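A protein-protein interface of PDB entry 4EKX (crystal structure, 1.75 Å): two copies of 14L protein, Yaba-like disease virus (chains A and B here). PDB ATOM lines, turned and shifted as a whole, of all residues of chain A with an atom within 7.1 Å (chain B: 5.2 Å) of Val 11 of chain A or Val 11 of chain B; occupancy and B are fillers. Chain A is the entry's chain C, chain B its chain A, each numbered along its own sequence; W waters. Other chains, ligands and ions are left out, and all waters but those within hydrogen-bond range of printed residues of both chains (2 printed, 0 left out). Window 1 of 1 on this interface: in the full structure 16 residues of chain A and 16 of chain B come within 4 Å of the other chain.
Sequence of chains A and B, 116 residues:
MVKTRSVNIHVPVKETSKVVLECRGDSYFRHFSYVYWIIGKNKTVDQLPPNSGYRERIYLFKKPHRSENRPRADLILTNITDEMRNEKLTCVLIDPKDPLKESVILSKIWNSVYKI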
ATOM      1  N   ASN A   8       9.797 -36.133   3.393  1.00  0.00           N
ATOM      2  CA  ASN A   8       9.502 -34.950   2.608  1.00  0.00           C
ATOM      3  C   ASN A   8      10.002 -33.717   3.320  1.00  0.00           C
ATOM      4  O   ASN A   8       9.975 -33.597   4.551  1.00  0.00           O
ATOM      5  CB  ASN A   8       8.018 -34.820   2.225  1.00  0.00           C
ATOM      6  CG  ASN A   8       7.803 -34.096   0.870  1.00  0.00           C
ATOM      7  OD1 ASN A   8       8.727 -33.499   0.301  1.00  0.00           O
ATOM      8  ND2 ASN A   8       6.569 -34.147   0.363  1.00  0.00           N
ATOM      9  N   ILE A   9      10.545 -32.829   2.505  1.00  0.00           N
ATOM     10  CA  ILE A   9      11.115 -31.584   2.996  1.00  0.00           C
ATOM     11  C   ILE A   9      10.213 -30.472   2.522  1.00  0.00           C
ATOM     12  O   ILE A   9       9.834 -30.426   1.343  1.00  0.00           O
ATOM     13  CB  ILE A   9      12.519 -31.364   2.400  1.00  0.00           C
ATOM     14  CG1 ILE A   9      13.477 -32.480   2.831  1.00  0.00           C
ATOM     15  CG2 ILE A   9      13.051 -29.976   2.777  1.00  0.00           C
ATOM     16  CD1 ILE A   9      14.738 -32.559   1.960  1.00  0.00           C
ATOM     17  N   HIS A  10       9.843 -29.578   3.441  1.00  0.00           N
ATOM     18  CA  HIS A  10       9.168 -28.342   3.051  1.00  0.00           C
ATOM     19  C   HIS A  10      10.163 -27.209   3.136  1.00  0.00           C
ATOM     20  O   HIS A  10      10.872 -27.094   4.133  1.00  0.00           O
ATOM     21  CB  HIS A  10       7.973 -28.046   3.949  1.00  0.00           C
ATOM     22  CG  HIS A  10       6.721 -28.740   3.528  1.00  0.00           C
ATOM     23  ND1 HIS A  10       6.586 -30.111   3.572  1.00  0.00           N
ATOM     24  CD2 HIS A  10       5.558 -28.261   3.028  1.00  0.00           C
ATOM     25  CE1 HIS A  10       5.386 -30.445   3.132  1.00  0.00           C
ATOM     26  NE2 HIS A  10       4.740 -29.340   2.806  1.00  0.00           N
ATOM     27  N   VAL A  11      10.231 -26.393   2.086  1.00  0.00           N
ATOM     28  CA  VAL A  11      11.192 -25.285   2.033  1.00  0.00           C
ATOM     29  C   VAL A  11      10.483 -23.973   1.741  1.00  0.00           C
ATOM     30  O   VAL A  11       9.438 -23.953   1.087  1.00  0.00           O
ATOM     31  CB  VAL A  11      12.255 -25.506   0.933  1.00  0.00           C
ATOM     32  CG1 VAL A  11      13.065 -26.765   1.226  1.00  0.00           C
ATOM     33  CG2 VAL A  11      11.584 -25.610  -0.426  1.00  0.00           C
ATOM     34  N   PRO A  12      11.058 -22.861   2.204  1.00  0.00           N
ATOM     35  CA  PRO A  12      10.384 -21.591   1.916  1.00  0.00           C
ATOM     36  C   PRO A  12      10.639 -21.179   0.470  1.00  0.00           C
ATOM     37  O   PRO A  12      11.712 -21.467  -0.062  1.00  0.00           O
ATOM     38  CB  PRO A  12      11.064 -20.613   2.886  1.00  0.00           C
ATOM     39  CG  PRO A  12      12.435 -21.198   3.103  1.00  0.00           C
ATOM     40  CD  PRO A  12      12.244 -22.693   3.068  1.00  0.00           C
ATOM     41  N   VAL A  13       9.671 -20.519  -0.158  1.00  0.00           N
ATOM     42  CA  VAL A  13       9.832 -20.124  -1.552  1.00  0.00           C
ATOM     43  C   VAL A  13      10.810 -18.966  -1.718  1.00  0.00           C
ATOM     44  O   VAL A  13      11.278 -18.702  -2.819  1.00  0.00           O
ATOM     45  CB  VAL A  13       8.478 -19.787  -2.226  1.00  0.00           C
ATOM     46  CG1 VAL A  13       7.551 -21.000  -2.169  1.00  0.00           C
ATOM     47  CG2 VAL A  13       7.833 -18.569  -1.572  1.00  0.00           C
ATOM     48  N   LYS A  14      11.122 -18.276  -0.623  1.00  0.00           N
ATOM     49  CA  LYS A  14      12.099 -17.200  -0.675  1.00  0.00           C
ATOM     50  C   LYS A  14      13.038 -17.243   0.521  1.00  0.00           C
ATOM     51  O   LYS A  14      12.661 -17.671   1.612  1.00  0.00           O
ATOM     52  CB  LYS A  14      11.405 -15.839  -0.728  1.00  0.00           C
ATOM     53  CG  LYS A  14      10.576 -15.521   0.500  1.00  0.00           C
ATOM     54  CD  LYS A  14       9.933 -14.154   0.355  1.00  0.00           C
ATOM     55  CE  LYS A  14       8.728 -14.014   1.262  1.00  0.00           C
ATOM     56  NZ  LYS A  14       9.081 -14.293   2.671  1.00  0.00           N
ATOM     57  N   VAL A  19      16.096 -18.979   7.846  1.00  0.00           N
ATOM     58  CA  VAL A  19      15.430 -19.923   6.953  1.00  0.00           C
ATOM     59  C   VAL A  19      15.172 -21.227   7.694  1.00  0.00           C
ATOM     60  O   VAL A  19      16.060 -21.756   8.361  1.00  0.00           O
ATOM     61  CB  VAL A  19      16.271 -20.167   5.678  1.00  0.00           C
ATOM     62  CG1 VAL A  19      15.882 -21.508   4.990  1.00  0.00           C
ATOM     63  CG2 VAL A  19      16.143 -18.980   4.730  1.00  0.00           C
ATOM     64  N   VAL A  20      13.950 -21.741   7.600  1.00  0.00           N
ATOM     65  CA  VAL A  20      13.637 -23.011   8.254  1.00  0.00           C
ATOM     66  C   VAL A  20      13.233 -24.062   7.216  1.00  0.00           C
ATOM     67  O   VAL A  20      12.325 -23.832   6.406  1.00  0.00           O
ATOM     68  CB  VAL A  20      12.504 -22.865   9.288  1.00  0.00           C
ATOM     69  CG1 VAL A  20      12.224 -24.212   9.950  1.00  0.00           C
ATOM     70  CG2 VAL A  20      12.868 -21.796  10.336  1.00  0.00           C
ATOM     71  N   LEU A  21      13.913 -25.205   7.224  1.00  0.00           N
ATOM     72  CA  LEU A  21      13.515 -26.312   6.368  1.00  0.00           C
ATOM     73  C   LEU A  21      12.875 -27.363   7.261  1.00  0.00           C
ATOM     74  O   LEU A  21      13.429 -27.738   8.296  1.00  0.00           O
ATOM     75  CB  LEU A  21      14.711 -26.916   5.619  1.00  0.00           C
ATOM     76  CG  LEU A  21      15.768 -25.961   5.056  1.00  0.00           C
ATOM     77  CD1 LEU A  21      16.819 -26.795   4.317  1.00  0.00           C
ATOM     78  CD2 LEU A  21      15.164 -24.924   4.128  1.00  0.00           C
ATOM     79  N   GLU A  22      11.709 -27.846   6.858  1.00  0.00           N
ATOM     80  CA  GLU A  22      10.974 -28.771   7.698  1.00  0.00           C
ATOM     81  C   GLU A  22      11.070 -30.156   7.112  1.00  0.00           C
ATOM     82  O   GLU A  22      10.578 -30.384   6.016  1.00  0.00           O
ATOM     83  CB  GLU A  22       9.510 -28.361   7.735  1.00  0.00           C
ATOM     84  CG  GLU A  22       9.322 -26.933   8.232  1.00  0.00           C
ATOM     85  CD  GLU A  22       7.924 -26.407   8.010  1.00  0.00           C
ATOM     86  OE1 GLU A  22       7.139 -27.075   7.311  1.00  0.00           O
ATOM     87  OE2 GLU A  22       7.616 -25.316   8.534  1.00  0.00           O
ATOM     88  N   TRP A  37      19.019 -34.400   9.900  1.00  0.00           N
ATOM     89  CA  TRP A  37      19.644 -33.788   8.737  1.00  0.00           C
ATOM     90  C   TRP A  37      21.114 -34.147   8.605  1.00  0.00           C
ATOM     91  O   TRP A  37      21.831 -34.339   9.593  1.00  0.00           O
ATOM     92  CB  TRP A  37      19.500 -32.249   8.800  1.00  0.00           C
ATOM     93  CG  TRP A  37      18.098 -31.769   8.515  1.00  0.00           C
ATOM     94  CD1 TRP A  37      17.089 -31.569   9.424  1.00  0.00           C
ATOM     95  CD2 TRP A  37      17.559 -31.417   7.235  1.00  0.00           C
ATOM     96  NE1 TRP A  37      15.952 -31.138   8.779  1.00  0.00           N
ATOM     97  CE2 TRP A  37      16.217 -31.033   7.435  1.00  0.00           C
ATOM     98  CE3 TRP A  37      18.085 -31.383   5.936  1.00  0.00           C
ATOM     99  CZ2 TRP A  37      15.395 -30.605   6.390  1.00  0.00           C
ATOM    100  CZ3 TRP A  37      17.267 -30.983   4.896  1.00  0.00           C
ATOM    101  CH2 TRP A  37      15.932 -30.598   5.128  1.00  0.00           C
ATOM    102  N   VAL A 104      17.790 -31.386  -0.827  1.00  0.00           N
ATOM    103  CA  VAL A 104      17.465 -30.135  -1.497  1.00  0.00           C
ATOM    104  C   VAL A 104      18.710 -29.267  -1.571  1.00  0.00           C
ATOM    105  O   VAL A 104      19.587 -29.341  -0.700  1.00  0.00           O
ATOM    106  CB  VAL A 104      16.316 -29.362  -0.774  1.00  0.00           C
ATOM    107  CG1 VAL A 104      16.697 -29.043   0.671  1.00  0.00           C
ATOM    108  CG2 VAL A 104      15.948 -28.073  -1.540  1.00  0.00           C
ATOM    109  N   LEU A 106      19.111 -25.297  -1.875  1.00  0.00           N
ATOM    110  CA  LEU A 106      18.238 -24.136  -1.776  1.00  0.00           C
ATOM    111  C   LEU A 106      18.334 -23.168  -2.954  1.00  0.00           C
ATOM    112  O   LEU A 106      17.328 -22.606  -3.383  1.00  0.00           O
ATOM    113  CB  LEU A 106      18.498 -23.395  -0.457  1.00  0.00           C
ATOM    114  CG  LEU A 106      18.169 -24.216   0.793  1.00  0.00           C
ATOM    115  CD1 LEU A 106      18.624 -23.490   2.071  1.00  0.00           C
ATOM    116  CD2 LEU A 106      16.671 -24.500   0.838  1.00  0.00           C
ATOM    117  N   ILE A 109      15.936 -23.976  -5.598  1.00  0.00           N
ATOM    118  CA  ILE A 109      14.572 -23.603  -5.245  1.00  0.00           C
ATOM    119  C   ILE A 109      14.340 -22.111  -5.464  1.00  0.00           C
ATOM    120  O   ILE A 109      13.377 -21.703  -6.116  1.00  0.00           O
ATOM    121  CB  ILE A 109      14.275 -23.928  -3.765  1.00  0.00           C
ATOM    122  CG1 ILE A 109      14.365 -25.439  -3.519  1.00  0.00           C
ATOM    123  CG2 ILE A 109      12.908 -23.354  -3.356  1.00  0.00           C
ATOM    124  CD1 ILE A 109      13.321 -26.243  -4.258  1.00  0.00           C
ATOM    125  N   TRP A 110      15.233 -21.303  -4.919  1.00  0.00           N
ATOM    126  CA  TRP A 110      15.052 -19.874  -4.899  1.00  0.00           C
ATOM    127  C   TRP A 110      15.236 -19.198  -6.227  1.00  0.00           C
ATOM    128  O   TRP A 110      14.708 -18.094  -6.451  1.00  0.00           O
ATOM    129  CB  TRP A 110      15.961 -19.260  -3.851  1.00  0.00           C
ATOM    130  CG  TRP A 110      15.594 -19.663  -2.447  1.00  0.00           C
ATOM    131  CD1 TRP A 110      14.352 -20.058  -1.979  1.00  0.00           C
ATOM    132  CD2 TRP A 110      16.472 -19.719  -1.278  1.00  0.00           C
ATOM    133  NE1 TRP A 110      14.403 -20.345  -0.646  1.00  0.00           N
ATOM    134  CE2 TRP A 110      15.642 -20.162  -0.165  1.00  0.00           C
ATOM    135  CE3 TRP A 110      17.809 -19.459  -1.053  1.00  0.00           C
ATOM    136  CZ2 TRP A 110      16.149 -20.329   1.103  1.00  0.00           C
ATOM    137  CZ3 TRP A 110      18.310 -19.628   0.232  1.00  0.00           C
ATOM    138  CH2 TRP A 110      17.498 -20.052   1.283  1.00  0.00           C
ATOM    139  N   ILE B   9       5.593 -18.688   2.438  1.00  0.00           N
ATOM    140  CA  ILE B   9       5.041 -19.984   2.014  1.00  0.00           C
ATOM    141  C   ILE B   9       6.100 -21.086   2.057  1.00  0.00           C
ATOM    142  O   ILE B   9       7.188 -20.945   1.493  1.00  0.00           O
ATOM    143  CB  ILE B   9       4.497 -19.923   0.564  1.00  0.00           C
ATOM    144  CG1 ILE B   9       3.384 -18.891   0.421  1.00  0.00           C
ATOM    145  CG2 ILE B   9       4.013 -21.316   0.090  1.00  0.00           C
ATOM    146  CD1 ILE B   9       2.939 -18.708  -1.029  1.00  0.00           C
ATOM    147  N   HIS B  10       5.795 -22.189   2.732  1.00  0.00           N
ATOM    148  CA  HIS B  10       6.638 -23.369   2.622  1.00  0.00           C
ATOM    149  C   HIS B  10       5.979 -24.357   1.678  1.00  0.00           C
ATOM    150  O   HIS B  10       4.777 -24.610   1.780  1.00  0.00           O
ATOM    151  CB  HIS B  10       6.850 -24.035   3.969  1.00  0.00           C
ATOM    152  CG  HIS B  10       7.906 -23.376   4.800  1.00  0.00           C
ATOM    153  ND1 HIS B  10       7.754 -22.107   5.326  1.00  0.00           N
ATOM    154  CD2 HIS B  10       9.134 -23.798   5.171  1.00  0.00           C
ATOM    155  CE1 HIS B  10       8.843 -21.788   6.006  1.00  0.00           C
ATOM    156  NE2 HIS B  10       9.696 -22.796   5.923  1.00  0.00           N
ATOM    157  N   VAL B  11       6.766 -24.900   0.756  1.00  0.00           N
ATOM    158  CA  VAL B  11       6.249 -25.882  -0.192  1.00  0.00           C
ATOM    159  C   VAL B  11       7.063 -27.168  -0.123  1.00  0.00           C
ATOM    160  O   VAL B  11       8.239 -27.149   0.255  1.00  0.00           O
ATOM    161  CB  VAL B  11       6.275 -25.354  -1.653  1.00  0.00           C
ATOM    162  CG1 VAL B  11       5.320 -24.175  -1.817  1.00  0.00           C
ATOM    163  CG2 VAL B  11       7.692 -24.965  -2.054  1.00  0.00           C
ATOM    164  N   PRO B  12       6.441 -28.300  -0.484  1.00  0.00           N
ATOM    165  CA  PRO B  12       7.243 -29.529  -0.511  1.00  0.00           C
ATOM    166  C   PRO B  12       8.131 -29.559  -1.756  1.00  0.00           C
ATOM    167  O   PRO B  12       7.710 -29.081  -2.819  1.00  0.00           O
ATOM    168  CB  PRO B  12       6.187 -30.634  -0.569  1.00  0.00           C
ATOM    169  CG  PRO B  12       5.029 -30.004  -1.305  1.00  0.00           C
ATOM    170  CD  PRO B  12       5.048 -28.519  -0.927  1.00  0.00           C
ATOM    171  N   VAL B  13       9.339 -30.099  -1.615  1.00  0.00           N
ATOM    172  CA  VAL B  13      10.295 -30.168  -2.718  1.00  0.00           C
ATOM    173  C   VAL B  13       9.856 -31.138  -3.811  1.00  0.00           C
ATOM    174  O   VAL B  13      10.343 -31.076  -4.937  1.00  0.00           O
ATOM    175  CB  VAL B  13      11.698 -30.566  -2.235  1.00  0.00           C
ATOM    176  CG1 VAL B  13      12.232 -29.519  -1.261  1.00  0.00           C
ATOM    177  CG2 VAL B  13      11.671 -31.938  -1.585  1.00  0.00           C
ATOM    178  N   VAL B  20       0.741 -30.352   0.605  1.00  0.00           N
ATOM    179  CA  VAL B  20       0.359 -29.302   1.545  1.00  0.00           C
ATOM    180  C   VAL B  20       1.304 -28.117   1.428  1.00  0.00           C
ATOM    181  O   VAL B  20       2.519 -28.288   1.497  1.00  0.00           O
ATOM    182  CB  VAL B  20       0.415 -29.801   3.003  1.00  0.00           C
ATOM    183  CG1 VAL B  20       0.034 -28.671   3.966  1.00  0.00           C
ATOM    184  CG2 VAL B  20      -0.498 -31.006   3.189  1.00  0.00           C
ATOM    185  N   LEU B  21       0.732 -26.931   1.217  1.00  0.00           N
ATOM    186  CA  LEU B  21       1.488 -25.685   1.250  1.00  0.00           C
ATOM    187  C   LEU B  21       1.123 -24.989   2.532  1.00  0.00           C
ATOM    188  O   LEU B  21      -0.055 -24.899   2.881  1.00  0.00           O
ATOM    189  CB  LEU B  21       1.126 -24.782   0.071  1.00  0.00           C
ATOM    190  CG  LEU B  21       0.964 -25.513  -1.280  1.00  0.00           C
ATOM    191  CD1 LEU B  21       0.710 -24.501  -2.389  1.00  0.00           C
ATOM    192  CD2 LEU B  21       2.189 -26.369  -1.595  1.00  0.00           C
ATOM    193  N   VAL B 104       3.312 -18.739  -5.458  1.00  0.00           N
ATOM    194  CA  VAL B 104       4.130 -19.832  -5.953  1.00  0.00           C
ATOM    195  C   VAL B 104       3.407 -20.538  -7.091  1.00  0.00           C
ATOM    196  O   VAL B 104       2.175 -20.614  -7.109  1.00  0.00           O
ATOM    197  CB  VAL B 104       4.467 -20.847  -4.823  1.00  0.00           C
ATOM    198  CG1 VAL B 104       3.197 -21.466  -4.250  1.00  0.00           C
ATOM    199  CG2 VAL B 104       5.421 -21.931  -5.331  1.00  0.00           C
ATOM    200  N   LEU B 106       3.756 -24.235  -8.488  1.00  0.00           N
ATOM    201  CA  LEU B 106       4.388 -25.488  -8.093  1.00  0.00           C
ATOM    202  C   LEU B 106       5.273 -26.146  -9.154  1.00  0.00           C
ATOM    203  O   LEU B 106       6.352 -26.634  -8.833  1.00  0.00           O
ATOM    204  CB  LEU B 106       3.339 -26.467  -7.552  1.00  0.00           C
ATOM    205  CG  LEU B 106       2.728 -25.912  -6.259  1.00  0.00           C
ATOM    206  CD1 LEU B 106       1.493 -26.700  -5.831  1.00  0.00           C
ATOM    207  CD2 LEU B 106       3.789 -25.891  -5.158  1.00  0.00           C
ATOM    208  N   ILE B 109       8.771 -25.074  -8.916  1.00  0.00           N
ATOM    209  CA  ILE B 109       9.517 -25.618  -7.803  1.00  0.00           C
ATOM    210  C   ILE B 109       9.899 -27.058  -8.094  1.00  0.00           C
ATOM    211  O   ILE B 109      11.031 -27.459  -7.887  1.00  0.00           O
ATOM    212  CB  ILE B 109       8.694 -25.582  -6.509  1.00  0.00           C
ATOM    213  CG1 ILE B 109       8.323 -24.144  -6.150  1.00  0.00           C
ATOM    214  CG2 ILE B 109       9.462 -26.238  -5.378  1.00  0.00           C
ATOM    215  CD1 ILE B 109       9.475 -23.341  -5.596  1.00  0.00           C
HETATM  216  O   HOH W   1       3.267 -31.820   0.951  1.00  0.00           O
HETATM  217  O   HOH W   2      11.821 -20.192   6.461  1.00  0.00           O
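Among the printed residues, merely in contact across the chains: His 10 of chain A with Val 11 of chain B, Val 11 of chain A with His 10 of chain B, Pro 12 of chain A with Ile 9 of chain B, Ile 9 of chain A with Pro 12 of chain B, His 10 of chain A with Pro 12 of chain B, Asn 8 of chain A with Pro 12 of chain B, Pro 12 of chain A with His 10 of chain B, Val 11 of chain A with Ile 9 of chain B, Val 11 of chain A with Val 13 of chain B, Ile 9 of chain A with Val 11 of chain B, Asn 8 of chain A with Val 13 of chain B, His 10 of chain A with His 10 of chain B, Val 13 of chain A with Val 11 of chain B, Val 13 of chain A with Val 104 of chain B, Glu 22 of chain A with His 10 of chain B and Val 104 of chain A with Val 13 of chain B.
Printed residues of chain A that touch a printed residue of chain B: Asn 8, Ile 9, His 10, Val 11, Pro 12, Val 13, Val 20, Glu 22 and Val 104.
Of the 10 printed residues of chain B, 7 touch a printed residue of chain A.
Among the printed residues, no Asp or Glu carboxylate lies within 4 Å of a Lys or Arg side-chain nitrogen of the other chain.
Ile 9 of chain A touches Val 13 of chain B, and with the chains exchanged Val 13 of chain A touches Ile 9 of chain B.
His 10 of chain A touches Val 11 of chain B, and with the chains exchanged Val 11 of chain A touches His 10 of chain B.
His 10 of chain A touches Val 20 of chain B, and with the chains exchanged Val 20 of chain A touches His 10 of chain B.
Val 13 of chain A touches Val 104 of chain B, and with the chains exchanged Val 104 of chain A touches Val 13 of chain B.
10 positions are printed for both chains.
Water W2 lies within hydrogen-bond range of the backbone NH of Val 20 of chain A and a ring nitrogen (NE2) of His 10 of chain B.
Water W1 lies within hydrogen-bond range of N of Val 20 of chain B (2.9 Å) and NE2 of His 10 of chain A (3.4 Å).
The backbone carbonyl oxygen (O) of Val 20 of chain B lies within hydrogen-bond range of a ring nitrogen (NE2) of His 10 of chain A (2.8 Å).
N of Val 11 of chain A lies within hydrogen-bond range of O of Val 11 of chain B (2.8 Å).
O of Ile 9 of chain A is in hydrogen-bond range of N of Val 13 of chain B (3.0 Å).
The backbone NH of Val 13 of chain A lies within hydrogen-bond range of the backbone carbonyl oxygen of Ile 9 of chain B, at 3.0 Å.
The backbone carbonyl oxygen (O) of Val 20 of chain A lies within hydrogen-bond range of a ring nitrogen (NE2) of His 10 of chain B, at 2.9 Å.
Val 11 of chain A touches just these residues of chain B: Ile 9, His 10, Val 11 and Val 13.
Of the printed residues of chain B, Ile 9 of chain A touches Val 11 (3.8 Å), Pro 12 (3.3 Å) and Val 13 (3.0 Å).
Of the printed residues of chain A, Pro 12 of chain B touches Asn 8, Ile 9 and His 10.
Of the printed residues of chain A, Val 13 of chain B touches Asn 8 (3.8 Å), Ile 9 (3.0 Å), Val 11 (3.8 Å) and Val 104 (3.997 Å).
Printed residues of chain B within 4 Å of Val 104 of chain A: Val 13.
Of the printed residues of chain B, Val 20 of chain A touches His 10 (2.9 Å).
Leu 106 of chain B touches none of the printed residues of chain A.
The nearest residue of chain B that does not touch Val 11 of chain A is Pro 12 of chain B (5.0 Å).
The nearest residue of chain A that does not touch Val 11 of chain B is Pro 12 of chain A (5.0 Å).
The backbone NH of His 10 of chain A sits at hydrogen-bond distance from the backbone carbonyl oxygen of Glu 22 of chain A (2.8 Å).
The backbone carbonyl oxygen (O) of Pro 12 of chain A lies within hydrogen-bond range of the indole nitrogen (NE1) of Trp 110 of chain A (3.0 Å).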
